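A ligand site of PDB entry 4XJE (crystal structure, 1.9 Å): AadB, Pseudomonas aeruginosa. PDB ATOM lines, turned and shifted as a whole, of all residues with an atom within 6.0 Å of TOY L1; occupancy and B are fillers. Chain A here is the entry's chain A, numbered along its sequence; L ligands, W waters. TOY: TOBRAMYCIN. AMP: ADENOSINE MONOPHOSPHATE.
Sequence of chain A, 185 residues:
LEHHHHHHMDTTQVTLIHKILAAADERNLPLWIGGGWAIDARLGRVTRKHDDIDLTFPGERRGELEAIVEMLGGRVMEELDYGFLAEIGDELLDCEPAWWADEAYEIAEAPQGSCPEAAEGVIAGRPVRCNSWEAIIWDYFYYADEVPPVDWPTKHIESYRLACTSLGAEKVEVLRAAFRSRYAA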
ATOM      1  N   ASP A  51      21.331  22.813 -11.493  1.00  0.00           N
ATOM      2  CA  ASP A  51      20.071  23.107 -12.175  1.00  0.00           C
ATOM      3  C   ASP A  51      18.910  22.437 -11.457  1.00  0.00           C
ATOM      4  O   ASP A  51      17.774  22.924 -11.493  1.00  0.00           O
ATOM      5  CB  ASP A  51      20.087  22.627 -13.626  1.00  0.00           C
ATOM      6  CG  ASP A  51      21.005  23.446 -14.514  1.00  0.00           C
ATOM      7  OD1 ASP A  51      21.543  24.470 -14.059  1.00  0.00           O
ATOM      8  OD2 ASP A  51      21.199  23.047 -15.688  1.00  0.00           O
ATOM      9  N   ASP A  52      19.195  21.304 -10.833  1.00  0.00           N
ATOM     10  CA  ASP A  52      18.155  20.492 -10.227  1.00  0.00           C
ATOM     11  C   ASP A  52      18.738  19.579  -9.165  1.00  0.00           C
ATOM     12  O   ASP A  52      19.939  19.633  -8.871  1.00  0.00           O
ATOM     13  CB  ASP A  52      17.444  19.669 -11.304  1.00  0.00           C
ATOM     14  CG  ASP A  52      18.409  18.862 -12.163  1.00  0.00           C
ATOM     15  OD1 ASP A  52      19.575  18.692 -11.779  1.00  0.00           O
ATOM     16  OD2 ASP A  52      17.976  18.385 -13.240  1.00  0.00           O
ATOM     17  N   ASP A  54      19.180  15.606  -8.391  1.00  0.00           N
ATOM     18  CA  ASP A  54      19.123  14.280  -8.965  1.00  0.00           C
ATOM     19  C   ASP A  54      18.985  13.246  -7.862  1.00  0.00           C
ATOM     20  O   ASP A  54      19.750  13.242  -6.901  1.00  0.00           O
ATOM     21  CB  ASP A  54      20.371  14.007  -9.811  1.00  0.00           C
ATOM     22  CG  ASP A  54      20.508  14.984 -10.955  1.00  0.00           C
ATOM     23  OD1 ASP A  54      19.635  14.968 -11.858  1.00  0.00           O
ATOM     24  OD2 ASP A  54      21.490  15.756 -10.958  1.00  0.00           O
ATOM     25  N   ASP A  81      13.098   9.288 -20.196  1.00  0.00           N
ATOM     26  CA  ASP A  81      13.609   8.084 -20.840  1.00  0.00           C
ATOM     27  C   ASP A  81      14.189   7.085 -19.834  1.00  0.00           C
ATOM     28  O   ASP A  81      14.158   5.869 -20.053  1.00  0.00           O
ATOM     29  CB  ASP A  81      14.675   8.428 -21.880  1.00  0.00           C
ATOM     30  CG  ASP A  81      14.094   9.008 -23.152  1.00  0.00           C
ATOM     31  OD1 ASP A  81      12.854   8.995 -23.312  1.00  0.00           O
ATOM     32  OD2 ASP A  81      14.877   9.482 -24.000  1.00  0.00           O
ATOM     33  N   TYR A  82      14.716   7.599 -18.722  1.00  0.00           N
ATOM     34  CA  TYR A  82      15.443   6.797 -17.736  1.00  0.00           C
ATOM     35  C   TYR A  82      14.787   6.827 -16.354  1.00  0.00           C
ATOM     36  O   TYR A  82      15.325   6.263 -15.409  1.00  0.00           O
ATOM     37  CB  TYR A  82      16.876   7.309 -17.618  1.00  0.00           C
ATOM     38  CG  TYR A  82      16.908   8.802 -17.457  1.00  0.00           C
ATOM     39  CD1 TYR A  82      16.676   9.385 -16.218  1.00  0.00           C
ATOM     40  CD2 TYR A  82      17.120   9.626 -18.549  1.00  0.00           C
ATOM     41  CE1 TYR A  82      16.678  10.748 -16.074  1.00  0.00           C
ATOM     42  CE2 TYR A  82      17.123  10.991 -18.414  1.00  0.00           C
ATOM     43  CZ  TYR A  82      16.903  11.555 -17.166  1.00  0.00           C
ATOM     44  OH  TYR A  82      16.918  12.917 -17.040  1.00  0.00           O
ATOM     45  N   ASP A  94      14.998  15.226 -10.667  1.00  0.00           N
ATOM     46  CA  ASP A  94      15.253  14.265 -11.726  1.00  0.00           C
ATOM     47  C   ASP A  94      15.495  12.892 -11.109  1.00  0.00           C
ATOM     48  O   ASP A  94      16.530  12.653 -10.484  1.00  0.00           O
ATOM     49  CB  ASP A  94      16.460  14.714 -12.555  1.00  0.00           C
ATOM     50  CG  ASP A  94      16.722  13.805 -13.738  1.00  0.00           C
ATOM     51  OD1 ASP A  94      17.310  12.727 -13.529  1.00  0.00           O
ATOM     52  OD2 ASP A  94      16.360  14.184 -14.865  1.00  0.00           O
ATOM     53  N   GLU A  96      15.727   8.695 -10.963  1.00  0.00           N
ATOM     54  CA  GLU A  96      16.079   7.490 -11.702  1.00  0.00           C
ATOM     55  C   GLU A  96      15.989   6.260 -10.808  1.00  0.00           C
ATOM     56  O   GLU A  96      16.515   6.263  -9.699  1.00  0.00           O
ATOM     57  CB  GLU A  96      17.493   7.604 -12.286  1.00  0.00           C
ATOM     58  CG  GLU A  96      17.897   6.428 -13.144  1.00  0.00           C
ATOM     59  CD  GLU A  96      19.180   6.663 -13.909  1.00  0.00           C
ATOM     60  OE1 GLU A  96      20.034   7.433 -13.412  1.00  0.00           O
ATOM     61  OE2 GLU A  96      19.336   6.077 -14.998  1.00  0.00           O
ATOM     62  N   ILE A 107      21.776   0.998 -10.675  1.00  0.00           N
ATOM     63  CA  ILE A 107      21.134   1.698 -11.774  1.00  0.00           C
ATOM     64  C   ILE A 107      21.331   0.903 -13.055  1.00  0.00           C
ATOM     65  O   ILE A 107      22.425   0.400 -13.310  1.00  0.00           O
ATOM     66  CB  ILE A 107      21.701   3.122 -11.939  1.00  0.00           C
ATOM     67  CG1 ILE A 107      21.435   3.955 -10.677  1.00  0.00           C
ATOM     68  CG2 ILE A 107      21.100   3.811 -13.156  1.00  0.00           C
ATOM     69  CD1 ILE A 107      22.360   5.137 -10.530  1.00  0.00           C
ATOM     70  N   ALA A 108      20.287   0.796 -13.863  1.00  0.00           N
ATOM     71  CA  ALA A 108      20.398   0.122 -15.142  1.00  0.00           C
ATOM     72  C   ALA A 108      21.373   0.871 -16.040  1.00  0.00           C
ATOM     73  O   ALA A 108      21.352   2.102 -16.087  1.00  0.00           O
ATOM     74  CB  ALA A 108      19.035   0.017 -15.808  1.00  0.00           C
ATOM     75  N   GLU A 109      22.224   0.122 -16.736  1.00  0.00           N
ATOM     76  CA  GLU A 109      23.217   0.712 -17.625  1.00  0.00           C
ATOM     77  C   GLU A 109      24.085   1.737 -16.907  1.00  0.00           C
ATOM     78  O   GLU A 109      24.183   2.894 -17.325  1.00  0.00           O
ATOM     79  CB  GLU A 109      22.541   1.365 -18.832  1.00  0.00           C
ATOM     80  CG  GLU A 109      21.742   0.400 -19.682  1.00  0.00           C
ATOM     81  CD  GLU A 109      20.945   1.111 -20.759  1.00  0.00           C
ATOM     82  OE1 GLU A 109      21.514   2.006 -21.425  1.00  0.00           O
ATOM     83  OE2 GLU A 109      19.746   0.778 -20.944  1.00  0.00           O
ATOM     84  N   ALA A 110      24.707   1.308 -15.808  1.00  0.00           N
ATOM     85  CA  ALA A 110      25.618   2.140 -15.040  1.00  0.00           C
ATOM     86  C   ALA A 110      26.682   1.250 -14.424  1.00  0.00           C
ATOM     87  O   ALA A 110      26.532   0.030 -14.410  1.00  0.00           O
ATOM     88  CB  ALA A 110      24.865   2.925 -13.967  1.00  0.00           C
ATOM     89  N   TRP A 138      30.296   8.299 -15.395  1.00  0.00           N
ATOM     90  CA  TRP A 138      29.619   7.530 -16.435  1.00  0.00           C
ATOM     91  C   TRP A 138      28.616   8.367 -17.223  1.00  0.00           C
ATOM     92  O   TRP A 138      28.523   8.256 -18.449  1.00  0.00           O
ATOM     93  CB  TRP A 138      28.919   6.329 -15.794  1.00  0.00           C
ATOM     94  CG  TRP A 138      28.287   5.345 -16.706  1.00  0.00           C
ATOM     95  CD1 TRP A 138      26.965   5.285 -17.057  1.00  0.00           C
ATOM     96  CD2 TRP A 138      28.922   4.230 -17.352  1.00  0.00           C
ATOM     97  NE1 TRP A 138      26.751   4.207 -17.899  1.00  0.00           N
ATOM     98  CE2 TRP A 138      27.939   3.550 -18.088  1.00  0.00           C
ATOM     99  CE3 TRP A 138      30.238   3.751 -17.371  1.00  0.00           C
ATOM    100  CZ2 TRP A 138      28.219   2.419 -18.850  1.00  0.00           C
ATOM    101  CZ3 TRP A 138      30.523   2.629 -18.131  1.00  0.00           C
ATOM    102  CH2 TRP A 138      29.515   1.971 -18.858  1.00  0.00           C
ATOM    103  N   ASP A 139      27.872   9.214 -16.530  1.00  0.00           N
ATOM    104  CA  ASP A 139      26.849  10.024 -17.182  1.00  0.00           C
ATOM    105  C   ASP A 139      27.447  11.128 -18.045  1.00  0.00           C
ATOM    106  O   ASP A 139      26.790  11.617 -18.966  1.00  0.00           O
ATOM    107  CB  ASP A 139      25.888  10.613 -16.152  1.00  0.00           C
ATOM    108  CG  ASP A 139      24.799   9.636 -15.739  1.00  0.00           C
ATOM    109  OD1 ASP A 139      24.583   8.629 -16.457  1.00  0.00           O
ATOM    110  OD2 ASP A 139      24.134   9.877 -14.707  1.00  0.00           O
ATOM    111  N   TYR A 142      27.855   9.739 -21.781  1.00  0.00           N
ATOM    112  CA  TYR A 142      26.670   9.968 -22.613  1.00  0.00           C
ATOM    113  C   TYR A 142      26.635  11.395 -23.118  1.00  0.00           C
ATOM    114  O   TYR A 142      26.401  11.659 -24.300  1.00  0.00           O
ATOM    115  CB  TYR A 142      25.375   9.711 -21.833  1.00  0.00           C
ATOM    116  CG  TYR A 142      25.132   8.304 -21.372  1.00  0.00           C
ATOM    117  CD1 TYR A 142      24.706   7.313 -22.243  1.00  0.00           C
ATOM    118  CD2 TYR A 142      25.292   7.976 -20.029  1.00  0.00           C
ATOM    119  CE1 TYR A 142      24.458   6.025 -21.794  1.00  0.00           C
ATOM    120  CE2 TYR A 142      25.057   6.693 -19.577  1.00  0.00           C
ATOM    121  CZ  TYR A 142      24.643   5.723 -20.463  1.00  0.00           C
ATOM    122  OH  TYR A 142      24.417   4.462 -19.984  1.00  0.00           O
ATOM    123  N   TYR A 143      26.852  12.322 -22.186  1.00  0.00           N
ATOM    124  CA  TYR A 143      26.800  13.751 -22.455  1.00  0.00           C
ATOM    125  C   TYR A 143      27.769  14.106 -23.574  1.00  0.00           C
ATOM    126  O   TYR A 143      27.445  14.904 -24.458  1.00  0.00           O
ATOM    127  CB  TYR A 143      27.124  14.524 -21.175  1.00  0.00           C
ATOM    128  CG  TYR A 143      26.849  16.011 -21.211  1.00  0.00           C
ATOM    129  CD1 TYR A 143      26.012  16.584 -22.165  1.00  0.00           C
ATOM    130  CD2 TYR A 143      27.446  16.844 -20.270  1.00  0.00           C
ATOM    131  CE1 TYR A 143      25.784  17.949 -22.170  1.00  0.00           C
ATOM    132  CE2 TYR A 143      27.216  18.202 -20.287  1.00  0.00           C
ATOM    133  CZ  TYR A 143      26.386  18.747 -21.233  1.00  0.00           C
ATOM    134  OH  TYR A 143      26.163  20.098 -21.240  1.00  0.00           O
ATOM    135  N   GLU A 146      26.608  13.231 -27.098  1.00  0.00           N
ATOM    136  CA  GLU A 146      25.452  13.994 -27.588  1.00  0.00           C
ATOM    137  C   GLU A 146      25.779  15.468 -27.804  1.00  0.00           C
ATOM    138  O   GLU A 146      25.295  16.067 -28.764  1.00  0.00           O
ATOM    139  CB  GLU A 146      24.291  13.849 -26.607  1.00  0.00           C
ATOM    140  CG  GLU A 146      23.760  12.429 -26.527  1.00  0.00           C
ATOM    141  CD  GLU A 146      22.956  12.164 -25.266  1.00  0.00           C
ATOM    142  OE1 GLU A 146      22.796  10.983 -24.905  1.00  0.00           O
ATOM    143  OE2 GLU A 146      22.491  13.145 -24.639  1.00  0.00           O
ATOM    144  N   TYR A 183      28.599  -0.001 -25.760  1.00  0.00           N
ATOM    145  CA  TYR A 183      27.682   0.695 -26.647  1.00  0.00           C
ATOM    146  C   TYR A 183      28.087   0.639 -28.125  1.00  0.00           C
ATOM    147  O   TYR A 183      27.348   1.117 -28.981  1.00  0.00           O
ATOM    148  CB  TYR A 183      27.546   2.147 -26.196  1.00  0.00           C
ATOM    149  CG  TYR A 183      26.658   2.261 -24.971  1.00  0.00           C
ATOM    150  CD1 TYR A 183      25.315   1.935 -25.050  1.00  0.00           C
ATOM    151  CD2 TYR A 183      27.168   2.677 -23.755  1.00  0.00           C
ATOM    152  CE1 TYR A 183      24.505   2.019 -23.939  1.00  0.00           C
ATOM    153  CE2 TYR A 183      26.362   2.770 -22.642  1.00  0.00           C
ATOM    154  CZ  TYR A 183      25.018   2.438 -22.742  1.00  0.00           C
ATOM    155  OH  TYR A 183      24.197   2.520 -21.644  1.00  0.00           O
HETATM  156  C11 TOY L   1      22.043   8.627 -18.574  1.00  0.00           C
HETATM  157  O11 TOY L   1      20.982   9.325 -17.950  1.00  0.00           O
HETATM  158  C21 TOY L   1      21.835   8.668 -20.078  1.00  0.00           C
HETATM  159  N21 TOY L   1      21.745  10.054 -20.589  1.00  0.00           N
HETATM  160  C31 TOY L   1      20.584   7.865 -20.423  1.00  0.00           C
HETATM  161  C41 TOY L   1      20.654   6.446 -19.880  1.00  0.00           C
HETATM  162  O41 TOY L   1      19.422   5.785 -20.147  1.00  0.00           O
HETATM  163  C51 TOY L   1      20.919   6.494 -18.381  1.00  0.00           C
HETATM  164  O51 TOY L   1      22.098   7.294 -18.113  1.00  0.00           O
HETATM  165  C61 TOY L   1      21.185   5.111 -17.813  1.00  0.00           C
HETATM  166  N61 TOY L   1      21.461   5.123 -16.370  1.00  0.00           N
HETATM  167  C12 TOY L   1      20.025  11.939 -14.877  1.00  0.00           C
HETATM  168  N12 TOY L   1      20.002  12.901 -13.771  1.00  0.00           N
HETATM  169  C22 TOY L   1      20.803  10.678 -14.495  1.00  0.00           C
HETATM  170  C32 TOY L   1      20.792   9.663 -15.637  1.00  0.00           C
HETATM  171  N32 TOY L   1      21.594   8.487 -15.277  1.00  0.00           N
HETATM  172  C42 TOY L   1      21.307  10.283 -16.939  1.00  0.00           C
HETATM  173  C52 TOY L   1      20.572  11.571 -17.288  1.00  0.00           C
HETATM  174  O52 TOY L   1      21.155  12.155 -18.448  1.00  0.00           O
HETATM  175  C62 TOY L   1      20.662  12.544 -16.126  1.00  0.00           C
HETATM  176  O62 TOY L   1      19.940  13.730 -16.458  1.00  0.00           O
HETATM  177  C13 TOY L   1      20.699  14.860 -16.850  1.00  0.00           C
HETATM  178  C23 TOY L   1      20.175  16.080 -16.113  1.00  0.00           C
HETATM  179  O23 TOY L   1      20.155  15.834 -14.710  1.00  0.00           O
HETATM  180  C33 TOY L   1      18.766  16.461 -16.593  1.00  0.00           C
HETATM  181  N33 TOY L   1      18.310  17.689 -15.924  1.00  0.00           N
HETATM  182  C43 TOY L   1      18.816  16.630 -18.106  1.00  0.00           C
HETATM  183  O43 TOY L   1      17.522  16.941 -18.616  1.00  0.00           O
HETATM  184  C53 TOY L   1      19.300  15.315 -18.712  1.00  0.00           C
HETATM  185  O53 TOY L   1      20.618  15.040 -18.253  1.00  0.00           O
HETATM  186  C63 TOY L   1      19.347  15.325 -20.221  1.00  0.00           C
HETATM  187  O63 TOY L   1      19.716  14.051 -20.730  1.00  0.00           O
HETATM  188  P   AMP L   2      22.753  17.965 -13.250  1.00  0.00           P
HETATM  189  O1P AMP L   2      21.365  17.442 -12.936  1.00  0.00           O
HETATM  190  O2P AMP L   2      22.593  19.256 -14.051  1.00  0.00           O
HETATM  191  O3P AMP L   2      23.629  17.991 -12.045  1.00  0.00           O
HETATM  192  O5' AMP L   2      23.368  16.900 -14.264  1.00  0.00           O
HETATM  193  C5' AMP L   2      23.790  15.621 -13.812  1.00  0.00           C
HETATM  194  C4' AMP L   2      24.661  14.947 -14.833  1.00  0.00           C
HETATM  195  O4' AMP L   2      23.881  14.651 -16.012  1.00  0.00           O
HETATM  196  C3' AMP L   2      25.820  15.770 -15.350  1.00  0.00           C
HETATM  197  O3' AMP L   2      26.938  15.731 -14.468  1.00  0.00           O
HETATM  198  C2' AMP L   2      26.103  15.148 -16.709  1.00  0.00           C
HETATM  199  O2' AMP L   2      26.905  13.987 -16.574  1.00  0.00           O
HETATM  200  C1' AMP L   2      24.705  14.718 -17.157  1.00  0.00           C
HETATM  201  N9  AMP L   2      24.104  15.660 -18.125  1.00  0.00           N
HETATM  202  C8  AMP L   2      23.839  16.994 -17.947  1.00  0.00           C
HETATM  203  N7  AMP L   2      23.299  17.575 -18.994  1.00  0.00           N
HETATM  204  C5  AMP L   2      23.189  16.549 -19.921  1.00  0.00           C
HETATM  205  C6  AMP L   2      22.695  16.517 -21.236  1.00  0.00           C
HETATM  206  N6  AMP L   2      22.198  17.584 -21.872  1.00  0.00           N
HETATM  207  N1  AMP L   2      22.734  15.337 -21.889  1.00  0.00           N
HETATM  208  C2  AMP L   2      23.233  14.271 -21.262  1.00  0.00           C
HETATM  209  N3  AMP L   2      23.732  14.185 -20.027  1.00  0.00           N
HETATM  210  C4  AMP L   2      23.687  15.365 -19.406  1.00  0.00           C
HETATM  211  O   HOH W   1      22.278  12.637 -12.195  1.00  0.00           O
HETATM  212  O   HOH W   2      23.868   6.332 -15.650  1.00  0.00           O
HETATM  213  O   HOH W   3      24.057  11.475 -19.202  1.00  0.00           O
HETATM  214  O   HOH W   4      18.505  11.235 -11.643  1.00  0.00           O
HETATM  215  O   HOH W   5      20.877  19.716 -16.090  1.00  0.00           O
HETATM  216  O   HOH W   6      17.447  18.861 -20.577  1.00  0.00           O
HETATM  217  O   HOH W   7      17.504   7.070 -21.490  1.00  0.00           O
HETATM  218  O   HOH W   8      19.436  11.217 -21.061  1.00  0.00           O
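OE1 of Glu 96 is in salt-bridge range of N32 of TOY L1 (2.7 Å). An oxygen (O1P) of AMP L2 lies close to the side-chain carboxylate (OD1) of Asp 52 (2.5 Å). An oxygen (O2') of AMP L2 sits close to the backbone carbonyl oxygen (O) of Asp 139 (3.4 Å). A nitrogen (N12) of TOY L1 is in salt-bridge range of the side-chain carboxylate (OD1) of Asp 54 (2.8 Å). An oxygen (O1P) of AMP L2 lies close to the side-chain carboxylate of Asp 54 (2.6 Å). OD2 of Asp 52 lies within salt-bridge range of N33 of TOY L1 (2.8 Å). The backbone carbonyl oxygen (O) of Ala 108 sits at hydrogen-bond distance from a nitrogen (N61) of TOY L1 (3.0 Å). N12 of TOY L1 lies within salt-bridge range of OD1 of Asp 94 (2.7 Å). The side-chain carboxylate of Asp 139 lies within salt-bridge range of a nitrogen (N32) of TOY L1 (3.0 Å). O62 of TOY L1 is in hydrogen-bond range of OH of Tyr 82 (3.2 Å).
An oxygen (O23) of TOY L1 is in hydrogen-bond range of an oxygen (O1P) of AMP L2 (2.7 Å).
OE1 of Glu 109 sits at hydrogen-bond distance from OH of Tyr 183 (2.7 Å). The backbone carbonyl oxygen of Glu 109 lies within hydrogen-bond range of the indole nitrogen of Trp 138 (2.9 Å). The side-chain hydroxyl (OH) of Tyr 142 sits at hydrogen-bond distance from the side-chain hydroxyl (OH) of Tyr 183 (2.6 Å). The side-chain hydroxyl (OH) of Tyr 142 is in hydrogen-bond range of the backbone carbonyl oxygen (O) of Glu 109, 3.1 Å away. The indole nitrogen of Trp 138 is in hydrogen-bond range of the side-chain hydroxyl of Tyr 142. The side-chain carboxylate (OD2) of Asp 94 lies within hydrogen-bond range of the side-chain hydroxyl (OH) of Tyr 82.
CG2 of Ile 107 touches N61 of TOY L1 (3.5 Å). Glu 109 touches TOY L1 (O to N61, 3.6 Å). Tyr 142 touches TOY L1. Hydrophobic or aromatic side chains that line TOY L1: Tyr 82, Ile 107 and Tyr 142.
Water W1 bridges a nitrogen (N12) of TOY L1 (2.8 Å) and the side-chain carboxylate of Asp 54 (3.4 Å). Water W2 lies within hydrogen-bond range of the side-chain carboxylate (OD1) of Asp 139 (2.5 Å) and a nitrogen (N61) of TOY L1 (2.8 Å). Water W3 lies within hydrogen-bond range of the backbone carbonyl oxygen of Asp 139 (2.7 Å), a nitrogen (N3) of AMP L2 (2.9 Å) and a nitrogen (N21) of TOY L1 (3.0 Å). Water W4 lies within hydrogen-bond range of OD1 of Asp 94 (2.7 Å) and N12 of TOY L1 (3.1 Å). Water W5 lies within hydrogen-bond range of O2P of AMP L2 (2.7 Å), N33 of TOY L1 (3.3 Å) and OD2 of Asp 51 (3.4 Å).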
